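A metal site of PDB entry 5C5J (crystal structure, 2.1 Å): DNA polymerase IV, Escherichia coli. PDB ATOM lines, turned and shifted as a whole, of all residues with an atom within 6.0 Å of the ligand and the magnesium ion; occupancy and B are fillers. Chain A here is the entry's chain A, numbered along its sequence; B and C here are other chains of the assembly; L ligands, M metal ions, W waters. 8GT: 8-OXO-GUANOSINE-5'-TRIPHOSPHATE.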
ATOM      1  N   ASP A   9     -10.687  -2.638   8.374  1.00  0.00           N
ATOM      2  CA  ASP A   9     -11.884  -2.473   7.564  1.00  0.00           C
ATOM      3  C   ASP A   9     -11.558  -2.885   6.131  1.00  0.00           C
ATOM      4  O   ASP A   9     -10.813  -2.180   5.449  1.00  0.00           O
ATOM      5  CB  ASP A   9     -12.373  -1.019   7.633  1.00  0.00           C
ATOM      6  CG  ASP A   9     -13.745  -0.805   6.992  1.00  0.00           C
ATOM      7  OD1 ASP A   9     -14.061  -1.477   5.987  1.00  0.00           O
ATOM      8  OD2 ASP A   9     -14.515   0.056   7.492  1.00  0.00           O
ATOM      9  N   MET A  10     -12.126  -3.999   5.665  1.00  0.00           N
ATOM     10  CA  MET A  10     -11.922  -4.426   4.285  1.00  0.00           C
ATOM     11  C   MET A  10     -12.504  -3.422   3.295  1.00  0.00           C
ATOM     12  O   MET A  10     -13.568  -2.845   3.523  1.00  0.00           O
ATOM     13  CB  MET A  10     -12.559  -5.796   4.056  1.00  0.00           C
ATOM     14  CG  MET A  10     -12.162  -6.879   5.055  1.00  0.00           C
ATOM     15  SD  MET A  10     -10.436  -7.346   4.883  1.00  0.00           S
ATOM     16  CE  MET A  10     -10.309  -7.581   3.114  1.00  0.00           C
ATOM     17  N   ASP A  11     -11.824  -3.239   2.157  1.00  0.00           N
ATOM     18  CA  ASP A  11     -12.211  -2.270   1.146  1.00  0.00           C
ATOM     19  C   ASP A  11     -13.197  -2.912   0.173  1.00  0.00           C
ATOM     20  O   ASP A  11     -12.897  -3.942  -0.425  1.00  0.00           O
ATOM     21  CB  ASP A  11     -10.984  -1.772   0.381  1.00  0.00           C
ATOM     22  CG  ASP A  11      -9.887  -1.235   1.295  1.00  0.00           C
ATOM     23  OD1 ASP A  11     -10.164  -0.293   2.057  1.00  0.00           O
ATOM     24  OD2 ASP A  11      -8.756  -1.742   1.245  1.00  0.00           O
ATOM     25  N   CYS A  12     -14.378  -2.286   0.014  1.00  0.00           N
ATOM     26  CA  CYS A  12     -15.412  -2.764  -0.900  1.00  0.00           C
ATOM     27  C   CYS A  12     -15.608  -4.277  -0.792  1.00  0.00           C
ATOM     28  O   CYS A  12     -15.576  -5.019  -1.778  1.00  0.00           O
ATOM     29  CB  CYS A  12     -15.097  -2.366  -2.349  1.00  0.00           C
ATOM     30  SG  CYS A  12     -14.972  -0.601  -2.507  1.00  0.00           S
ATOM     31  N   PHE A  13     -15.841  -4.729   0.440  1.00  0.00           N
ATOM     32  CA  PHE A  13     -15.686  -6.137   0.778  1.00  0.00           C
ATOM     33  C   PHE A  13     -16.328  -7.044  -0.266  1.00  0.00           C
ATOM     34  O   PHE A  13     -15.634  -7.852  -0.897  1.00  0.00           O
ATOM     35  CB  PHE A  13     -16.245  -6.415   2.165  1.00  0.00           C
ATOM     36  CG  PHE A  13     -15.995  -7.805   2.632  1.00  0.00           C
ATOM     37  CD1 PHE A  13     -14.749  -8.394   2.434  1.00  0.00           C
ATOM     38  CD2 PHE A  13     -16.977  -8.528   3.275  1.00  0.00           C
ATOM     39  CE1 PHE A  13     -14.498  -9.670   2.859  1.00  0.00           C
ATOM     40  CE2 PHE A  13     -16.735  -9.819   3.705  1.00  0.00           C
ATOM     41  CZ  PHE A  13     -15.492 -10.386   3.504  1.00  0.00           C
ATOM     42  N   PHE A  14     -17.644  -6.912  -0.498  1.00  0.00           N
ATOM     43  CA  PHE A  14     -18.322  -7.869  -1.372  1.00  0.00           C
ATOM     44  C   PHE A  14     -17.811  -7.760  -2.801  1.00  0.00           C
ATOM     45  O   PHE A  14     -17.622  -8.778  -3.473  1.00  0.00           O
ATOM     46  CB  PHE A  14     -19.839  -7.691  -1.352  1.00  0.00           C
ATOM     47  CG  PHE A  14     -20.504  -8.004  -0.026  1.00  0.00           C
ATOM     48  CD1 PHE A  14     -19.781  -8.507   1.053  1.00  0.00           C
ATOM     49  CD2 PHE A  14     -21.865  -7.807   0.131  1.00  0.00           C
ATOM     50  CE1 PHE A  14     -20.407  -8.788   2.256  1.00  0.00           C
ATOM     51  CE2 PHE A  14     -22.499  -8.086   1.323  1.00  0.00           C
ATOM     52  CZ  PHE A  14     -21.777  -8.577   2.396  1.00  0.00           C
ATOM     53  N   ALA A  15     -17.593  -6.544  -3.306  1.00  0.00           N
ATOM     54  CA  ALA A  15     -17.121  -6.389  -4.678  1.00  0.00           C
ATOM     55  C   ALA A  15     -15.664  -6.804  -4.833  1.00  0.00           C
ATOM     56  O   ALA A  15     -15.274  -7.306  -5.892  1.00  0.00           O
ATOM     57  CB  ALA A  15     -17.309  -4.944  -5.137  1.00  0.00           C
ATOM     58  N   ILE A  42     -28.666  -1.627  -3.524  1.00  0.00           N
ATOM     59  CA  ILE A  42     -27.242  -1.942  -3.644  1.00  0.00           C
ATOM     60  C   ILE A  42     -26.683  -2.247  -2.259  1.00  0.00           C
ATOM     61  O   ILE A  42     -26.877  -1.456  -1.329  1.00  0.00           O
ATOM     62  CB  ILE A  42     -26.478  -0.792  -4.309  1.00  0.00           C
ATOM     63  CG1 ILE A  42     -27.091  -0.446  -5.663  1.00  0.00           C
ATOM     64  CG2 ILE A  42     -24.984  -1.141  -4.443  1.00  0.00           C
ATOM     65  CD1 ILE A  42     -27.182  -1.648  -6.599  1.00  0.00           C
ATOM     66  N   SER A  43     -25.985  -3.378  -2.127  1.00  0.00           N
ATOM     67  CA  SER A  43     -25.231  -3.665  -0.904  1.00  0.00           C
ATOM     68  C   SER A  43     -23.912  -2.886  -0.895  1.00  0.00           C
ATOM     69  O   SER A  43     -23.556  -2.297   0.126  1.00  0.00           O
ATOM     70  CB  SER A  43     -24.937  -5.169  -0.781  1.00  0.00           C
ATOM     71  OG  SER A  43     -25.884  -5.856   0.023  1.00  0.00           O
ATOM     72  N   THR A  44     -23.183  -2.921  -2.004  1.00  0.00           N
ATOM     73  CA  THR A  44     -21.911  -2.222  -2.163  1.00  0.00           C
ATOM     74  C   THR A  44     -21.527  -2.223  -3.641  1.00  0.00           C
ATOM     75  O   THR A  44     -22.098  -2.962  -4.446  1.00  0.00           O
ATOM     76  CB  THR A  44     -20.802  -2.858  -1.313  1.00  0.00           C
ATOM     77  OG1 THR A  44     -19.586  -2.110  -1.492  1.00  0.00           O
ATOM     78  CG2 THR A  44     -20.555  -4.289  -1.742  1.00  0.00           C
ATOM     79  N   ALA A  45     -20.539  -1.405  -3.974  1.00  0.00           N
ATOM     80  CA  ALA A  45     -20.086  -1.252  -5.350  1.00  0.00           C
ATOM     81  C   ALA A  45     -18.581  -1.033  -5.365  1.00  0.00           C
ATOM     82  O   ALA A  45     -17.986  -0.618  -4.371  1.00  0.00           O
ATOM     83  CB  ALA A  45     -20.801  -0.092  -6.047  1.00  0.00           C
ATOM     84  N   TYR A  47     -14.998   0.768  -6.987  1.00  0.00           N
ATOM     85  CA  TYR A  47     -14.686   2.172  -7.232  1.00  0.00           C
ATOM     86  C   TYR A  47     -15.071   2.644  -8.636  1.00  0.00           C
ATOM     87  O   TYR A  47     -15.497   3.803  -8.763  1.00  0.00           O
ATOM     88  CB  TYR A  47     -13.213   2.452  -6.924  1.00  0.00           C
ATOM     89  CG  TYR A  47     -12.966   2.625  -5.433  1.00  0.00           C
ATOM     90  CD1 TYR A  47     -13.218   3.841  -4.808  1.00  0.00           C
ATOM     91  CD2 TYR A  47     -12.532   1.560  -4.638  1.00  0.00           C
ATOM     92  CE1 TYR A  47     -13.018   4.004  -3.437  1.00  0.00           C
ATOM     93  CE2 TYR A  47     -12.319   1.719  -3.277  1.00  0.00           C
ATOM     94  CZ  TYR A  47     -12.567   2.934  -2.675  1.00  0.00           C
ATOM     95  OH  TYR A  47     -12.362   3.095  -1.325  1.00  0.00           O
ATOM     96  N   ARG A  50     -18.608   3.687  -8.109  1.00  0.00           N
ATOM     97  CA  ARG A  50     -18.807   4.864  -7.254  1.00  0.00           C
ATOM     98  C   ARG A  50     -18.460   6.162  -7.959  1.00  0.00           C
ATOM     99  O   ARG A  50     -18.906   7.221  -7.532  1.00  0.00           O
ATOM    100  CB  ARG A  50     -17.977   4.764  -5.990  1.00  0.00           C
ATOM    101  CG  ARG A  50     -18.082   3.469  -5.261  1.00  0.00           C
ATOM    102  CD  ARG A  50     -17.614   3.645  -3.848  1.00  0.00           C
ATOM    103  NE  ARG A  50     -17.236   2.388  -3.246  1.00  0.00           N
ATOM    104  CZ  ARG A  50     -18.037   1.671  -2.479  1.00  0.00           C
ATOM    105  NH1 ARG A  50     -19.283   2.096  -2.248  1.00  0.00           N
ATOM    106  NH2 ARG A  50     -17.608   0.521  -1.957  1.00  0.00           N
ATOM    107  N   SER A  56     -23.782   2.404  -1.329  1.00  0.00           N
ATOM    108  CA  SER A  56     -24.527   1.464  -0.512  1.00  0.00           C
ATOM    109  C   SER A  56     -25.878   2.037  -0.129  1.00  0.00           C
ATOM    110  O   SER A  56     -26.026   3.248   0.073  1.00  0.00           O
ATOM    111  CB  SER A  56     -23.736   1.111   0.733  1.00  0.00           C
ATOM    112  OG  SER A  56     -22.592   0.369   0.384  1.00  0.00           O
ATOM    113  N   ALA A  57     -26.879   1.157  -0.050  1.00  0.00           N
ATOM    114  CA  ALA A  57     -28.259   1.437   0.344  1.00  0.00           C
ATOM    115  C   ALA A  57     -29.041   2.139  -0.750  1.00  0.00           C
ATOM    116  O   ALA A  57     -30.243   2.372  -0.591  1.00  0.00           O
ATOM    117  CB  ALA A  57     -28.365   2.267   1.636  1.00  0.00           C
ATOM    118  N   SER A 102     -19.096  -6.566  11.909  1.00  0.00           N
ATOM    119  CA  SER A 102     -19.752  -7.045  10.698  1.00  0.00           C
ATOM    120  C   SER A 102     -18.837  -8.130  10.160  1.00  0.00           C
ATOM    121  O   SER A 102     -17.849  -8.485  10.823  1.00  0.00           O
ATOM    122  CB  SER A 102     -19.971  -5.910   9.699  1.00  0.00           C
ATOM    123  OG  SER A 102     -18.746  -5.523   9.085  1.00  0.00           O
ATOM    124  N   ASP A 104     -16.733  -7.789   7.790  1.00  0.00           N
ATOM    125  CA  ASP A 104     -15.476  -7.268   7.276  1.00  0.00           C
ATOM    126  C   ASP A 104     -14.894  -6.157   8.144  1.00  0.00           C
ATOM    127  O   ASP A 104     -14.001  -5.424   7.688  1.00  0.00           O
ATOM    128  CB  ASP A 104     -15.654  -6.785   5.850  1.00  0.00           C
ATOM    129  CG  ASP A 104     -16.403  -5.469   5.776  1.00  0.00           C
ATOM    130  OD1 ASP A 104     -17.424  -5.296   6.478  1.00  0.00           O
ATOM    131  OD2 ASP A 104     -15.937  -4.592   5.016  1.00  0.00           O
ATOM    132  N   GLU A 105     -15.360  -5.973   9.370  1.00  0.00           N
ATOM    133  CA  GLU A 105     -14.849  -4.934  10.243  1.00  0.00           C
ATOM    134  C   GLU A 105     -14.630  -5.503  11.629  1.00  0.00           C
ATOM    135  O   GLU A 105     -15.386  -6.377  12.080  1.00  0.00           O
ATOM    136  CB  GLU A 105     -15.821  -3.721  10.336  1.00  0.00           C
ATOM    137  CG  GLU A 105     -16.092  -2.986   9.030  1.00  0.00           C
ATOM    138  CD  GLU A 105     -16.856  -1.685   9.251  1.00  0.00           C
ATOM    139  OE1 GLU A 105     -17.167  -1.385  10.435  1.00  0.00           O
ATOM    140  OE2 GLU A 105     -17.135  -0.970   8.262  1.00  0.00           O
ATOM    141  N   ASP A 155     -10.976   5.144   7.661  1.00  0.00           N
ATOM    142  CA  ASP A 155     -11.494   5.669   6.413  1.00  0.00           C
ATOM    143  C   ASP A 155     -10.585   6.724   5.773  1.00  0.00           C
ATOM    144  O   ASP A 155     -10.738   7.015   4.588  1.00  0.00           O
ATOM    145  CB  ASP A 155     -12.886   6.250   6.632  1.00  0.00           C
ATOM    146  CG  ASP A 155     -13.932   5.178   6.878  1.00  0.00           C
ATOM    147  OD1 ASP A 155     -13.882   4.129   6.206  1.00  0.00           O
ATOM    148  OD2 ASP A 155     -14.796   5.374   7.762  1.00  0.00           O
ATOM    149  N   LYS A 158      -8.281   5.369   2.743  1.00  0.00           N
ATOM    150  CA  LYS A 158      -8.901   4.267   2.004  1.00  0.00           C
ATOM    151  C   LYS A 158      -8.846   4.534   0.512  1.00  0.00           C
ATOM    152  O   LYS A 158      -9.002   5.669   0.086  1.00  0.00           O
ATOM    153  CB  LYS A 158     -10.352   4.102   2.437  1.00  0.00           C
ATOM    154  CG  LYS A 158     -10.702   2.707   2.811  1.00  0.00           C
ATOM    155  CD  LYS A 158     -12.173   2.526   3.095  1.00  0.00           C
ATOM    156  CE  LYS A 158     -12.421   1.124   3.642  1.00  0.00           C
ATOM    157  NZ  LYS A 158     -12.361   1.113   5.132  1.00  0.00           N
ATOM    158  N   PRO A 159      -8.646   3.481  -0.293  1.00  0.00           N
ATOM    159  CA  PRO A 159      -8.448   2.084   0.131  1.00  0.00           C
ATOM    160  C   PRO A 159      -6.983   1.705   0.328  1.00  0.00           C
ATOM    161  O   PRO A 159      -6.078   2.435  -0.084  1.00  0.00           O
ATOM    162  CB  PRO A 159      -9.042   1.300  -1.042  1.00  0.00           C
ATOM    163  CG  PRO A 159      -8.698   2.147  -2.210  1.00  0.00           C
ATOM    164  CD  PRO A 159      -8.788   3.580  -1.748  1.00  0.00           C
ATOM    165  P    DA B   4     -35.994  -1.677   0.692  1.00  0.00           P
ATOM    166  OP1  DA B   4     -37.411  -2.104   0.527  1.00  0.00           O
ATOM    167  OP2  DA B   4     -35.661  -0.894   1.884  1.00  0.00           O
ATOM    168  O5'  DA B   4     -35.043  -2.950   0.540  1.00  0.00           O
ATOM    169  C5'  DA B   4     -35.120  -3.779  -0.604  1.00  0.00           C
ATOM    170  C4'  DA B   4     -34.531  -5.150  -0.301  1.00  0.00           C
ATOM    171  O4'  DA B   4     -33.127  -5.011   0.051  1.00  0.00           O
ATOM    172  C3'  DA B   4     -35.160  -5.851   0.887  1.00  0.00           C
ATOM    173  O3'  DA B   4     -35.071  -7.265   0.726  1.00  0.00           O
ATOM    174  C2'  DA B   4     -34.323  -5.361   2.062  1.00  0.00           C
ATOM    175  C1'  DA B   4     -32.940  -5.236   1.429  1.00  0.00           C
ATOM    176  N9   DA B   4     -32.168  -4.135   1.971  1.00  0.00           N
ATOM    177  C8   DA B   4     -32.662  -2.936   2.372  1.00  0.00           C
ATOM    178  N7   DA B   4     -31.746  -2.120   2.831  1.00  0.00           N
ATOM    179  C5   DA B   4     -30.571  -2.819   2.709  1.00  0.00           C
ATOM    180  C6   DA B   4     -29.240  -2.499   3.026  1.00  0.00           C
ATOM    181  N6   DA B   4     -28.865  -1.312   3.528  1.00  0.00           N
ATOM    182  N1   DA B   4     -28.293  -3.438   2.790  1.00  0.00           N
ATOM    183  C2   DA B   4     -28.678  -4.614   2.280  1.00  0.00           C
ATOM    184  N3   DA B   4     -29.897  -5.030   1.940  1.00  0.00           N
ATOM    185  C4   DA B   4     -30.807  -4.077   2.188  1.00  0.00           C
ATOM    186  P    DG B   5     -35.774  -8.218   1.813  1.00  0.00           P
ATOM    187  OP1  DG B   5     -36.209  -9.419   1.103  1.00  0.00           O
ATOM    188  OP2  DG B   5     -36.781  -7.437   2.587  1.00  0.00           O
ATOM    189  O5'  DG B   5     -34.596  -8.530   2.834  1.00  0.00           O
ATOM    190  C5'  DG B   5     -33.502  -9.324   2.415  1.00  0.00           C
ATOM    191  C4'  DG B   5     -32.518  -9.446   3.539  1.00  0.00           C
ATOM    192  O4'  DG B   5     -31.923  -8.158   3.785  1.00  0.00           O
ATOM    193  C3'  DG B   5     -33.147  -9.863   4.873  1.00  0.00           C
ATOM    194  O3'  DG B   5     -32.386 -10.890   5.444  1.00  0.00           O
ATOM    195  C2'  DG B   5     -33.100  -8.591   5.711  1.00  0.00           C
ATOM    196  C1'  DG B   5     -31.856  -7.940   5.161  1.00  0.00           C
ATOM    197  N9   DG B   5     -31.768  -6.503   5.399  1.00  0.00           N
ATOM    198  C8   DG B   5     -32.783  -5.577   5.360  1.00  0.00           C
ATOM    199  N7   DG B   5     -32.373  -4.351   5.600  1.00  0.00           N
ATOM    200  C5   DG B   5     -31.001  -4.482   5.807  1.00  0.00           C
ATOM    201  C6   DG B   5     -30.020  -3.498   6.114  1.00  0.00           C
ATOM    202  O6   DG B   5     -30.157  -2.288   6.264  1.00  0.00           O
ATOM    203  N1   DG B   5     -28.761  -4.066   6.252  1.00  0.00           N
ATOM    204  C2   DG B   5     -28.483  -5.402   6.115  1.00  0.00           C
ATOM    205  N2   DG B   5     -27.202  -5.759   6.285  1.00  0.00           N
ATOM    206  N3   DG B   5     -29.385  -6.319   5.824  1.00  0.00           N
ATOM    207  C4   DG B   5     -30.617  -5.788   5.686  1.00  0.00           C
ATOM    208  P    DC C  18     -20.819   1.723   9.427  1.00  0.00           P
ATOM    209  OP1  DC C  18     -19.393   1.934   9.713  1.00  0.00           O
ATOM    210  OP2  DC C  18     -21.484   2.598   8.439  1.00  0.00           O
ATOM    211  O5'  DC C  18     -21.001   0.200   8.948  1.00  0.00           O
ATOM    212  C5'  DC C  18     -20.756  -0.885   9.829  1.00  0.00           C
ATOM    213  C4'  DC C  18     -21.083  -2.197   9.132  1.00  0.00           C
ATOM    214  O4'  DC C  18     -22.511  -2.438   9.192  1.00  0.00           O
ATOM    215  C3'  DC C  18     -20.709  -2.199   7.651  1.00  0.00           C
ATOM    216  C2'  DC C  18     -21.868  -2.921   6.937  1.00  0.00           C
ATOM    217  C1'  DC C  18     -22.979  -2.991   7.975  1.00  0.00           C
ATOM    218  N1   DC C  18     -24.238  -2.281   7.569  1.00  0.00           N
ATOM    219  C2   DC C  18     -25.351  -3.018   7.159  1.00  0.00           C
ATOM    220  O2   DC C  18     -25.265  -4.253   7.134  1.00  0.00           O
ATOM    221  N3   DC C  18     -26.484  -2.368   6.789  1.00  0.00           N
ATOM    222  C4   DC C  18     -26.546  -1.033   6.824  1.00  0.00           C
ATOM    223  N4   DC C  18     -27.694  -0.434   6.465  1.00  0.00           N
ATOM    224  C5   DC C  18     -25.421  -0.252   7.243  1.00  0.00           C
ATOM    225  C6   DC C  18     -24.303  -0.907   7.587  1.00  0.00           C
HETATM  226  PG  8GT L   1     -15.524   0.503   2.090  1.00  0.00           P
HETATM  227  O1G 8GT L   1     -15.236   0.047   3.509  1.00  0.00           O
HETATM  228  O2G 8GT L   1     -16.285   1.817   2.132  1.00  0.00           O
HETATM  229  O3G 8GT L   1     -14.246   0.654   1.291  1.00  0.00           O
HETATM  230  O3B 8GT L   1     -16.426  -0.647   1.304  1.00  0.00           O
HETATM  231  PB  8GT L   1     -17.362  -1.754   2.072  1.00  0.00           P
HETATM  232  O1B 8GT L   1     -18.291  -2.347   1.028  1.00  0.00           O
HETATM  233  O2B 8GT L   1     -16.531  -2.856   2.710  1.00  0.00           O
HETATM  234  O3A 8GT L   1     -18.163  -0.874   3.238  1.00  0.00           O
HETATM  235  PA  8GT L   1     -18.738  -1.401   4.697  1.00  0.00           P
HETATM  236  O1A 8GT L   1     -17.600  -1.762   5.649  1.00  0.00           O
HETATM  237  O2A 8GT L   1     -19.524  -0.262   5.317  1.00  0.00           O
HETATM  238  O5' 8GT L   1     -19.738  -2.694   4.417  1.00  0.00           O
HETATM  239  C5' 8GT L   1     -19.247  -4.005   4.437  1.00  0.00           C
HETATM  240  C4' 8GT L   1     -20.085  -4.874   3.729  1.00  0.00           C
HETATM  241  O4' 8GT L   1     -21.484  -4.882   4.298  1.00  0.00           O
HETATM  242  C3' 8GT L   1     -20.314  -4.400   2.206  1.00  0.00           C
HETATM  243  O3' 8GT L   1     -19.286  -5.004   1.290  1.00  0.00           O
HETATM  244  C2' 8GT L   1     -21.450  -4.771   1.884  1.00  0.00           C
HETATM  245  C1' 8GT L   1     -22.302  -5.050   3.297  1.00  0.00           C
HETATM  246  N9  8GT L   1     -23.425  -4.184   3.383  1.00  0.00           N
HETATM  247  C8  8GT L   1     -24.867  -4.638   3.421  1.00  0.00           C
HETATM  248  N7  8GT L   1     -25.719  -3.395   3.510  1.00  0.00           N
HETATM  249  C5  8GT L   1     -24.805  -2.275   3.525  1.00  0.00           C
HETATM  250  C6  8GT L   1     -25.107  -0.798   3.618  1.00  0.00           C
HETATM  251  O6  8GT L   1     -26.230  -0.425   3.681  1.00  0.00           O
HETATM  252  N1  8GT L   1     -24.012   0.172   3.619  1.00  0.00           N
HETATM  253  C2  8GT L   1     -22.621  -0.308   3.539  1.00  0.00           C
HETATM  254  N2  8GT L   1     -21.535   0.648   3.544  1.00  0.00           N
HETATM  255  N3  8GT L   1     -22.345  -1.760   3.452  1.00  0.00           N
HETATM  256  C4  8GT L   1     -23.450  -2.732   3.449  1.00  0.00           C
HETATM  257  O8  8GT L   1     -25.268  -5.757   3.367  1.00  0.00           O
HETATM  258 MG    MG M   1     -15.336  -2.331   4.608  1.00  0.00          MG
HETATM  259  O   HOH W   1     -20.122   1.208   0.681  1.00  0.00           O
HETATM  260  O   HOH W   2     -24.410   2.532   4.333  1.00  0.00           O
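OG of Ser 43 sits at hydrogen-bond distance from O8 of the ligand (3.4 Å). OG1 of Thr 44 is in hydrogen-bond range of O1B of the ligand (2.8 Å). N1 of DA 4 of chain B is in hydrogen-bond range of a nitrogen (N7) of the ligand. N of Phe 13 sits at hydrogen-bond distance from O1B of the ligand. N of Cys 12 lies within hydrogen-bond range of O3B of the ligand, at 2.9 Å. The backbone NH (N) of Phe 14 lies within hydrogen-bond range of an oxygen (O3') of the ligand, at 3.1 Å. O1G of the ligand is in salt-bridge range of NZ of Lys 158, at 3.5 Å. OG of Ser 56 sits close to N2 of the ligand, at 3.3 Å.
The side-chain hydroxyl of Ser 56 sits at hydrogen-bond distance from the backbone carbonyl oxygen of Ser 43, at 2.8 Å. N2 of DG 5 of chain B sits close to O2 of DC 18 of chain C (2.6 Å). NH2 of Arg 50 is in hydrogen-bond range of OG1 of Thr 44, at 3.3 Å. OG of Ser 102 sits at hydrogen-bond distance from N of Glu 105 (3.4 Å). SG of Cys 12 lies within hydrogen-bond range of O of Ala 45 (3.5 Å). NH2 of Arg 50 lies within hydrogen-bond range of SG of Cys 12, at 2.9 Å. The side-chain carboxylate of Asp 155 lies within salt-bridge range of the side-chain amino group of Lys 158 (3.5 Å). OD2 of Asp 9 lies within salt-bridge range of NZ of Lys 158, 3.4 Å away.
OE2 of Glu 105 lies close to O1A of the ligand (2.8 Å). N4 of DC 18 of chain C sits close to an oxygen (O6) of the ligand (3.1 Å). Asp 11 touches the ligand. Arg 50 touches the ligand (NH2 to O3B, 3.7 Å). CB of Ala 57 touches O6 of the ligand, 3.998 Å away. N2 of DG 5 of chain B touches O8 of the ligand, 3.5 Å away. Within 4 Å of the ligand: Asp 9, Met 10, Asp 11, Cys 12, Phe 13, Phe 14, Ser 43, Thr 44, Arg 50, Ser 56, Ala 57, Asp 104, Glu 105, Lys 158, DA 4 of chain B, DG 5 of chain B and DC 18 of chain C.
Three residues have an atom within 4 Å of the magnesium ion: Asp 9, Met 10 and Asp 104.
The magnesium ion is bound by OD1 of Asp 9 (2.1 Å), O of Met 10 (2.1 Å), O2B of the ligand (2.3 Å), OD2 of Asp 104 (2.4 Å) and O1A of the ligand (2.6 Å). Slightly farther from the magnesium ion lies O1G of the ligand (2.6 Å).
Water W1 lies within hydrogen-bond range of OG of Ser 56 (2.6 Å), NH1 of Arg 50 (3.2 Å) and N2 of the ligand (3.2 Å).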
